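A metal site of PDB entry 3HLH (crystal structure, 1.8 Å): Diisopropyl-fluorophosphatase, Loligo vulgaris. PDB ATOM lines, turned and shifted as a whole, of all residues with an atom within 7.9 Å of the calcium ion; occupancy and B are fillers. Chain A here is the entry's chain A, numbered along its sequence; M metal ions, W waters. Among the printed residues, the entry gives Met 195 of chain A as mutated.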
ATOM      1  N   GLY A  19      20.867  -8.126 -11.363  1.00  0.00           N
ATOM      2  CA  GLY A  19      19.569  -8.706 -11.656  1.00  0.00           C
ATOM      3  C   GLY A  19      19.337 -10.077 -11.055  1.00  0.00           C
ATOM      4  O   GLY A  19      18.497 -10.833 -11.543  1.00  0.00           O
ATOM      5  N   ALA A  20      20.090 -10.388  -9.998  1.00  0.00           N
ATOM      6  CA  ALA A  20      20.001 -11.677  -9.295  1.00  0.00           C
ATOM      7  C   ALA A  20      18.637 -12.363  -9.467  1.00  0.00           C
ATOM      8  O   ALA A  20      17.603 -11.812  -9.091  1.00  0.00           O
ATOM      9  CB  ALA A  20      20.287 -11.480  -7.812  1.00  0.00           C
ATOM     10  N   GLU A  21      18.660 -13.564 -10.039  1.00  0.00           N
ATOM     11  CA  GLU A  21      17.434 -14.311 -10.280  1.00  0.00           C
ATOM     12  C   GLU A  21      17.658 -15.812 -10.378  1.00  0.00           C
ATOM     13  O   GLU A  21      18.770 -16.307 -10.137  1.00  0.00           O
ATOM     14  CB  GLU A  21      16.792 -13.819 -11.582  1.00  0.00           C
ATOM     15  CG  GLU A  21      15.539 -12.981 -11.389  1.00  0.00           C
ATOM     16  CD  GLU A  21      14.275 -13.831 -11.298  1.00  0.00           C
ATOM     17  OE1 GLU A  21      14.374 -15.034 -10.981  1.00  0.00           O
ATOM     18  OE2 GLU A  21      13.185 -13.281 -11.543  1.00  0.00           O
ATOM     19  N   GLY A  22      16.592 -16.530 -10.717  1.00  0.00           N
ATOM     20  CA  GLY A  22      16.636 -17.973 -10.898  1.00  0.00           C
ATOM     21  C   GLY A  22      17.360 -18.838  -9.874  1.00  0.00           C
ATOM     22  O   GLY A  22      18.161 -19.691 -10.265  1.00  0.00           O
ATOM     23  N   PRO A  36      20.856 -11.980 -15.076  1.00  0.00           N
ATOM     24  CA  PRO A  36      20.359 -11.481 -16.359  1.00  0.00           C
ATOM     25  C   PRO A  36      20.737 -10.059 -16.745  1.00  0.00           C
ATOM     26  O   PRO A  36      20.809  -9.733 -17.940  1.00  0.00           O
ATOM     27  CB  PRO A  36      18.844 -11.655 -16.238  1.00  0.00           C
ATOM     28  CG  PRO A  36      18.599 -11.536 -14.768  1.00  0.00           C
ATOM     29  CD  PRO A  36      19.739 -12.352 -14.197  1.00  0.00           C
ATOM     30  N   ALA A  74      17.268 -15.838 -16.970  1.00  0.00           N
ATOM     31  CA  ALA A  74      16.472 -15.283 -15.889  1.00  0.00           C
ATOM     32  C   ALA A  74      15.795 -16.249 -14.928  1.00  0.00           C
ATOM     33  O   ALA A  74      15.469 -15.874 -13.809  1.00  0.00           O
ATOM     34  CB  ALA A  74      15.414 -14.348 -16.491  1.00  0.00           C
ATOM     35  N   GLY A  75      15.561 -17.490 -15.361  1.00  0.00           N
ATOM     36  CA  GLY A  75      14.899 -18.455 -14.497  1.00  0.00           C
ATOM     37  C   GLY A  75      15.470 -19.851 -14.696  1.00  0.00           C
ATOM     38  O   GLY A  75      15.958 -20.160 -15.784  1.00  0.00           O
ATOM     39  N   MET A  90      15.683 -14.570 -21.503  1.00  0.00           N
ATOM     40  CA  MET A  90      14.936 -13.470 -22.117  1.00  0.00           C
ATOM     41  C   MET A  90      15.346 -13.105 -23.545  1.00  0.00           C
ATOM     42  O   MET A  90      14.573 -12.459 -24.260  1.00  0.00           O
ATOM     43  CB  MET A  90      15.013 -12.224 -21.221  1.00  0.00           C
ATOM     44  CG  MET A  90      14.235 -12.348 -19.901  1.00  0.00           C
ATOM     45  SD  MET A  90      12.421 -12.237 -20.097  1.00  0.00           S
ATOM     46  CE  MET A  90      12.204 -10.446 -20.174  1.00  0.00           C
ATOM     47  N   CYS A 119      12.176 -16.055 -22.843  1.00  0.00           N
ATOM     48  CA  CYS A 119      11.550 -16.615 -21.649  1.00  0.00           C
ATOM     49  C   CYS A 119      12.092 -16.034 -20.330  1.00  0.00           C
ATOM     50  O   CYS A 119      13.234 -15.576 -20.269  1.00  0.00           O
ATOM     51  CB  CYS A 119      11.710 -18.126 -21.663  1.00  0.00           C
ATOM     52  SG  CYS A 119      10.925 -18.914 -23.114  1.00  0.00           S
ATOM     53  N   ASN A 120      11.266 -16.079 -19.286  1.00  0.00           N
ATOM     54  CA  ASN A 120      11.626 -15.528 -17.983  1.00  0.00           C
ATOM     55  C   ASN A 120      11.806 -16.564 -16.863  1.00  0.00           C
ATOM     56  O   ASN A 120      12.848 -16.583 -16.196  1.00  0.00           O
ATOM     57  CB  ASN A 120      10.580 -14.493 -17.554  1.00  0.00           C
ATOM     58  CG  ASN A 120      10.981 -13.747 -16.302  1.00  0.00           C
ATOM     59  OD1 ASN A 120      11.055 -14.319 -15.221  1.00  0.00           O
ATOM     60  ND2 ASN A 120      11.238 -12.453 -16.444  1.00  0.00           N
ATOM     61  N   ASP A 121      10.812 -17.407 -16.648  1.00  0.00           N
ATOM     62  CA  ASP A 121      10.892 -18.425 -15.597  1.00  0.00           C
ATOM     63  C   ASP A 121      10.217 -19.705 -16.090  1.00  0.00           C
ATOM     64  O   ASP A 121       9.529 -19.706 -17.112  1.00  0.00           O
ATOM     65  CB  ASP A 121      10.216 -17.928 -14.307  1.00  0.00           C
ATOM     66  CG  ASP A 121      10.825 -18.522 -13.040  1.00  0.00           C
ATOM     67  OD1 ASP A 121      11.698 -19.409 -13.141  1.00  0.00           O
ATOM     68  OD2 ASP A 121      10.447 -18.088 -11.925  1.00  0.00           O
ATOM     69  N   CYS A 122      10.415 -20.794 -15.359  1.00  0.00           N
ATOM     70  CA  CYS A 122       9.828 -22.063 -15.738  1.00  0.00           C
ATOM     71  C   CYS A 122       9.619 -22.968 -14.519  1.00  0.00           C
ATOM     72  O   CYS A 122      10.233 -22.757 -13.474  1.00  0.00           O
ATOM     73  CB  CYS A 122      10.702 -22.776 -16.786  1.00  0.00           C
ATOM     74  SG  CYS A 122      12.424 -23.069 -16.312  1.00  0.00           S
ATOM     75  N   THR A 133       7.238 -19.196 -18.856  1.00  0.00           N
ATOM     76  CA  THR A 133       6.661 -17.881 -19.110  1.00  0.00           C
ATOM     77  C   THR A 133       7.573 -17.192 -20.108  1.00  0.00           C
ATOM     78  O   THR A 133       8.798 -17.320 -20.033  1.00  0.00           O
ATOM     79  CB  THR A 133       6.563 -17.029 -17.831  1.00  0.00           C
ATOM     80  OG1 THR A 133       7.870 -16.840 -17.262  1.00  0.00           O
ATOM     81  CG2 THR A 133       5.659 -17.708 -16.816  1.00  0.00           C
ATOM     82  N   PRO A 135       7.622 -13.407 -21.411  1.00  0.00           N
ATOM     83  CA  PRO A 135       7.169 -12.020 -21.470  1.00  0.00           C
ATOM     84  C   PRO A 135       7.883 -11.170 -22.508  1.00  0.00           C
ATOM     85  O   PRO A 135       7.451 -10.058 -22.801  1.00  0.00           O
ATOM     86  CB  PRO A 135       7.441 -11.521 -20.058  1.00  0.00           C
ATOM     87  CG  PRO A 135       8.755 -12.197 -19.743  1.00  0.00           C
ATOM     88  CD  PRO A 135       8.537 -13.623 -20.269  1.00  0.00           C
ATOM     89  N   PHE A 173       3.225  -9.233 -19.523  1.00  0.00           N
ATOM     90  CA  PHE A 173       4.442  -9.621 -18.838  1.00  0.00           C
ATOM     91  C   PHE A 173       4.307 -10.770 -17.840  1.00  0.00           C
ATOM     92  O   PHE A 173       4.421 -10.584 -16.625  1.00  0.00           O
ATOM     93  CB  PHE A 173       5.098  -8.419 -18.155  1.00  0.00           C
ATOM     94  CG  PHE A 173       6.606  -8.529 -18.071  1.00  0.00           C
ATOM     95  CD1 PHE A 173       7.203  -9.301 -17.079  1.00  0.00           C
ATOM     96  CD2 PHE A 173       7.419  -7.887 -19.003  1.00  0.00           C
ATOM     97  CE1 PHE A 173       8.598  -9.447 -17.026  1.00  0.00           C
ATOM     98  CE2 PHE A 173       8.805  -8.012 -18.959  1.00  0.00           C
ATOM     99  CZ  PHE A 173       9.400  -8.793 -17.972  1.00  0.00           C
ATOM    100  N   PRO A 174       4.024 -11.983 -18.355  1.00  0.00           N
ATOM    101  CA  PRO A 174       3.895 -13.150 -17.475  1.00  0.00           C
ATOM    102  C   PRO A 174       5.285 -13.347 -16.861  1.00  0.00           C
ATOM    103  O   PRO A 174       6.288 -13.181 -17.557  1.00  0.00           O
ATOM    104  CB  PRO A 174       3.516 -14.268 -18.452  1.00  0.00           C
ATOM    105  CG  PRO A 174       4.120 -13.804 -19.762  1.00  0.00           C
ATOM    106  CD  PRO A 174       3.774 -12.349 -19.758  1.00  0.00           C
ATOM    107  N   ASN A 175       5.347 -13.699 -15.582  1.00  0.00           N
ATOM    108  CA  ASN A 175       6.639 -13.850 -14.938  1.00  0.00           C
ATOM    109  C   ASN A 175       6.795 -15.160 -14.174  1.00  0.00           C
ATOM    110  O   ASN A 175       7.290 -16.149 -14.714  1.00  0.00           O
ATOM    111  CB  ASN A 175       6.894 -12.659 -14.006  1.00  0.00           C
ATOM    112  CG  ASN A 175       8.377 -12.405 -13.775  1.00  0.00           C
ATOM    113  OD1 ASN A 175       9.147 -13.332 -13.567  1.00  0.00           O
ATOM    114  ND2 ASN A 175       8.786 -11.135 -13.810  1.00  0.00           N
ATOM    115  N   GLY A 176       6.377 -15.170 -12.914  1.00  0.00           N
ATOM    116  CA  GLY A 176       6.471 -16.379 -12.115  1.00  0.00           C
ATOM    117  C   GLY A 176       5.492 -17.424 -12.598  1.00  0.00           C
ATOM    118  O   GLY A 176       4.486 -17.094 -13.240  1.00  0.00           O
ATOM    119  N   ILE A 177       5.768 -18.679 -12.289  1.00  0.00           N
ATOM    120  CA  ILE A 177       4.905 -19.779 -12.692  1.00  0.00           C
ATOM    121  C   ILE A 177       5.111 -20.962 -11.737  1.00  0.00           C
ATOM    122  O   ILE A 177       6.202 -21.144 -11.179  1.00  0.00           O
ATOM    123  CB  ILE A 177       5.220 -20.191 -14.164  1.00  0.00           C
ATOM    124  CG1 ILE A 177       4.171 -21.182 -14.675  1.00  0.00           C
ATOM    125  CG2 ILE A 177       6.625 -20.770 -14.252  1.00  0.00           C
ATOM    126  CD1 ILE A 177       4.172 -21.341 -16.185  1.00  0.00           C
ATOM    127  N   MET A 195       2.702  -9.957 -13.916  1.00  0.00           N
ATOM    128  CA  MET A 195       3.290  -8.934 -13.062  1.00  0.00           C
ATOM    129  C   MET A 195       2.670  -7.545 -12.884  1.00  0.00           C
ATOM    130  O   MET A 195       2.158  -7.229 -11.812  1.00  0.00           O
ATOM    131  CB  MET A 195       4.779  -8.771 -13.423  1.00  0.00           C
ATOM    132  CG  MET A 195       5.527  -7.865 -12.473  1.00  0.00           C
ATOM    133  SD  MET A 195       7.284  -7.781 -12.836  1.00  0.00           S
ATOM    134  CE  MET A 195       7.960  -8.740 -11.485  1.00  0.00           C
ATOM    135  N   ALA A 228       3.897  -9.504  -8.875  1.00  0.00           N
ATOM    136  CA  ALA A 228       4.341 -10.876  -8.710  1.00  0.00           C
ATOM    137  C   ALA A 228       5.483 -11.244  -9.650  1.00  0.00           C
ATOM    138  O   ALA A 228       5.368 -11.066 -10.864  1.00  0.00           O
ATOM    139  CB  ALA A 228       3.170 -11.832  -8.922  1.00  0.00           C
ATOM    140  N   ASP A 229       6.572 -11.739  -9.074  1.00  0.00           N
ATOM    141  CA  ASP A 229       7.734 -12.169  -9.854  1.00  0.00           C
ATOM    142  C   ASP A 229       7.782 -13.694  -9.684  1.00  0.00           C
ATOM    143  O   ASP A 229       6.846 -14.381 -10.079  1.00  0.00           O
ATOM    144  CB  ASP A 229       9.022 -11.499  -9.327  1.00  0.00           C
ATOM    145  CG  ASP A 229      10.132 -11.468 -10.370  1.00  0.00           C
ATOM    146  OD1 ASP A 229      10.225 -12.427 -11.157  1.00  0.00           O
ATOM    147  OD2 ASP A 229      10.919 -10.487 -10.411  1.00  0.00           O
ATOM    148  N   GLY A 230       8.840 -14.220  -9.075  1.00  0.00           N
ATOM    149  CA  GLY A 230       8.967 -15.668  -8.879  1.00  0.00           C
ATOM    150  C   GLY A 230       8.087 -16.273  -7.797  1.00  0.00           C
ATOM    151  O   GLY A 230       7.695 -15.602  -6.852  1.00  0.00           O
ATOM    152  N   MET A 231       7.796 -17.564  -7.933  1.00  0.00           N
ATOM    153  CA  MET A 231       6.944 -18.261  -6.983  1.00  0.00           C
ATOM    154  C   MET A 231       7.306 -19.730  -6.761  1.00  0.00           C
ATOM    155  O   MET A 231       8.007 -20.329  -7.572  1.00  0.00           O
ATOM    156  CB  MET A 231       5.492 -18.185  -7.451  1.00  0.00           C
ATOM    157  CG  MET A 231       5.270 -18.761  -8.847  1.00  0.00           C
ATOM    158  SD  MET A 231       3.527 -18.736  -9.367  1.00  0.00           S
ATOM    159  CE  MET A 231       3.162 -16.994  -9.170  1.00  0.00           C
ATOM    160  N   TRP A 244       7.674  -8.067  -6.143  1.00  0.00           N
ATOM    161  CA  TRP A 244       8.683  -7.075  -6.503  1.00  0.00           C
ATOM    162  C   TRP A 244       8.194  -5.638  -6.349  1.00  0.00           C
ATOM    163  O   TRP A 244       7.226  -5.238  -6.989  1.00  0.00           O
ATOM    164  CB  TRP A 244       9.109  -7.293  -7.965  1.00  0.00           C
ATOM    165  CG  TRP A 244      10.394  -6.631  -8.402  1.00  0.00           C
ATOM    166  CD1 TRP A 244      11.589  -7.249  -8.640  1.00  0.00           C
ATOM    167  CD2 TRP A 244      10.594  -5.250  -8.744  1.00  0.00           C
ATOM    168  NE1 TRP A 244      12.512  -6.351  -9.118  1.00  0.00           N
ATOM    169  CE2 TRP A 244      11.926  -5.110  -9.192  1.00  0.00           C
ATOM    170  CE3 TRP A 244       9.775  -4.119  -8.723  1.00  0.00           C
ATOM    171  CZ2 TRP A 244      12.461  -3.885  -9.616  1.00  0.00           C
ATOM    172  CZ3 TRP A 244      10.301  -2.892  -9.145  1.00  0.00           C
ATOM    173  CH2 TRP A 244      11.635  -2.789  -9.593  1.00  0.00           C
ATOM    174  N   SER A 271      12.942 -10.780  -6.136  1.00  0.00           N
ATOM    175  CA  SER A 271      12.705 -11.215  -7.513  1.00  0.00           C
ATOM    176  C   SER A 271      12.293 -12.668  -7.603  1.00  0.00           C
ATOM    177  O   SER A 271      11.435 -13.034  -8.402  1.00  0.00           O
ATOM    178  CB  SER A 271      13.959 -10.974  -8.362  1.00  0.00           C
ATOM    179  OG  SER A 271      15.059 -11.726  -7.876  1.00  0.00           O
ATOM    180  N   ASN A 272      12.893 -13.522  -6.769  1.00  0.00           N
ATOM    181  CA  ASN A 272      12.567 -14.938  -6.812  1.00  0.00           C
ATOM    182  C   ASN A 272      12.956 -15.646  -5.515  1.00  0.00           C
ATOM    183  O   ASN A 272      13.571 -15.050  -4.634  1.00  0.00           O
ATOM    184  CB  ASN A 272      13.278 -15.596  -7.994  1.00  0.00           C
ATOM    185  CG  ASN A 272      12.424 -16.631  -8.688  1.00  0.00           C
ATOM    186  OD1 ASN A 272      11.697 -17.386  -8.040  1.00  0.00           O
ATOM    187  ND2 ASN A 272      12.514 -16.677 -10.009  1.00  0.00           N
ATOM    188  N   THR A 285      16.348 -14.033  -4.044  1.00  0.00           N
ATOM    189  CA  THR A 285      17.144 -13.157  -4.887  1.00  0.00           C
ATOM    190  C   THR A 285      16.390 -11.832  -4.908  1.00  0.00           C
ATOM    191  O   THR A 285      15.154 -11.827  -4.845  1.00  0.00           O
ATOM    192  CB  THR A 285      17.258 -13.687  -6.335  1.00  0.00           C
ATOM    193  OG1 THR A 285      15.945 -14.008  -6.819  1.00  0.00           O
ATOM    194  CG2 THR A 285      18.129 -14.931  -6.385  1.00  0.00           C
ATOM    195  N   HIS A 287      16.475  -7.406  -6.338  1.00  0.00           N
ATOM    196  CA  HIS A 287      17.067  -6.410  -7.209  1.00  0.00           C
ATOM    197  C   HIS A 287      17.405  -5.063  -6.606  1.00  0.00           C
ATOM    198  O   HIS A 287      17.883  -4.167  -7.310  1.00  0.00           O
ATOM    199  CB  HIS A 287      16.161  -6.234  -8.436  1.00  0.00           C
ATOM    200  CG  HIS A 287      16.029  -7.488  -9.258  1.00  0.00           C
ATOM    201  ND1 HIS A 287      15.027  -7.656 -10.199  1.00  0.00           N
ATOM    202  CD2 HIS A 287      16.782  -8.607  -9.297  1.00  0.00           C
ATOM    203  CE1 HIS A 287      15.182  -8.833 -10.775  1.00  0.00           C
ATOM    204  NE2 HIS A 287      16.233  -9.432 -10.246  1.00  0.00           N
HETATM  205 CA    CA M   1      11.305 -13.699 -12.877  1.00  0.00          CA
HETATM  206  O   HOH W   1      12.602 -15.649 -13.448  1.00  0.00           O
HETATM  207  O   HOH W   2       9.870 -15.391 -11.982  1.00  0.00           O
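The backbone carbonyl oxygen (O) of Asp 229 lies close to the backbone NH (N) of Gly 176, at 3.0 Å.
The backbone NH of Gly 75 sits at hydrogen-bond distance from the backbone carbonyl oxygen of Asn 120 (3.0 Å).
The side-chain hydroxyl (OG1) of Thr 133 sits at hydrogen-bond distance from the backbone carbonyl oxygen (O) of Asn 175 (2.7 Å).
OE1 of Glu 21 lies within hydrogen-bond range of ND2 of Asn 272, at 2.7 Å.
The backbone NH (N) of Asn 120 sits at hydrogen-bond distance from the backbone carbonyl oxygen (O) of Thr 133 (2.9 Å).
Of the 29 residues printed, 4 come within 4 Å of the calcium ion.
Along chain A the residues within 4 Å of the calcium ion span positions 21 to 229.
The nearest printed residue that does not touch the calcium ion is Asn 272 (4.3 Å).
The calcium ion is bound by OD1 of Asn 175.
OE2 of Glu 21 is bound to the calcium ion (2.3 Å).
Water W2 binds the calcium ion, 2.4 Å away.
The side-chain carboxylate (OD1) of Asp 229 binds the calcium ion, 2.4 Å away.
Water W1 is bound to the calcium ion, at 2.4 Å.
The calcium ion is bound by OD1 of Asn 120.
The calcium ion has six donor atoms within binding distance.
Water W2 bridges OD2 of Asp 121 (2.8 Å) and N of Gly 230 (3.3 Å).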
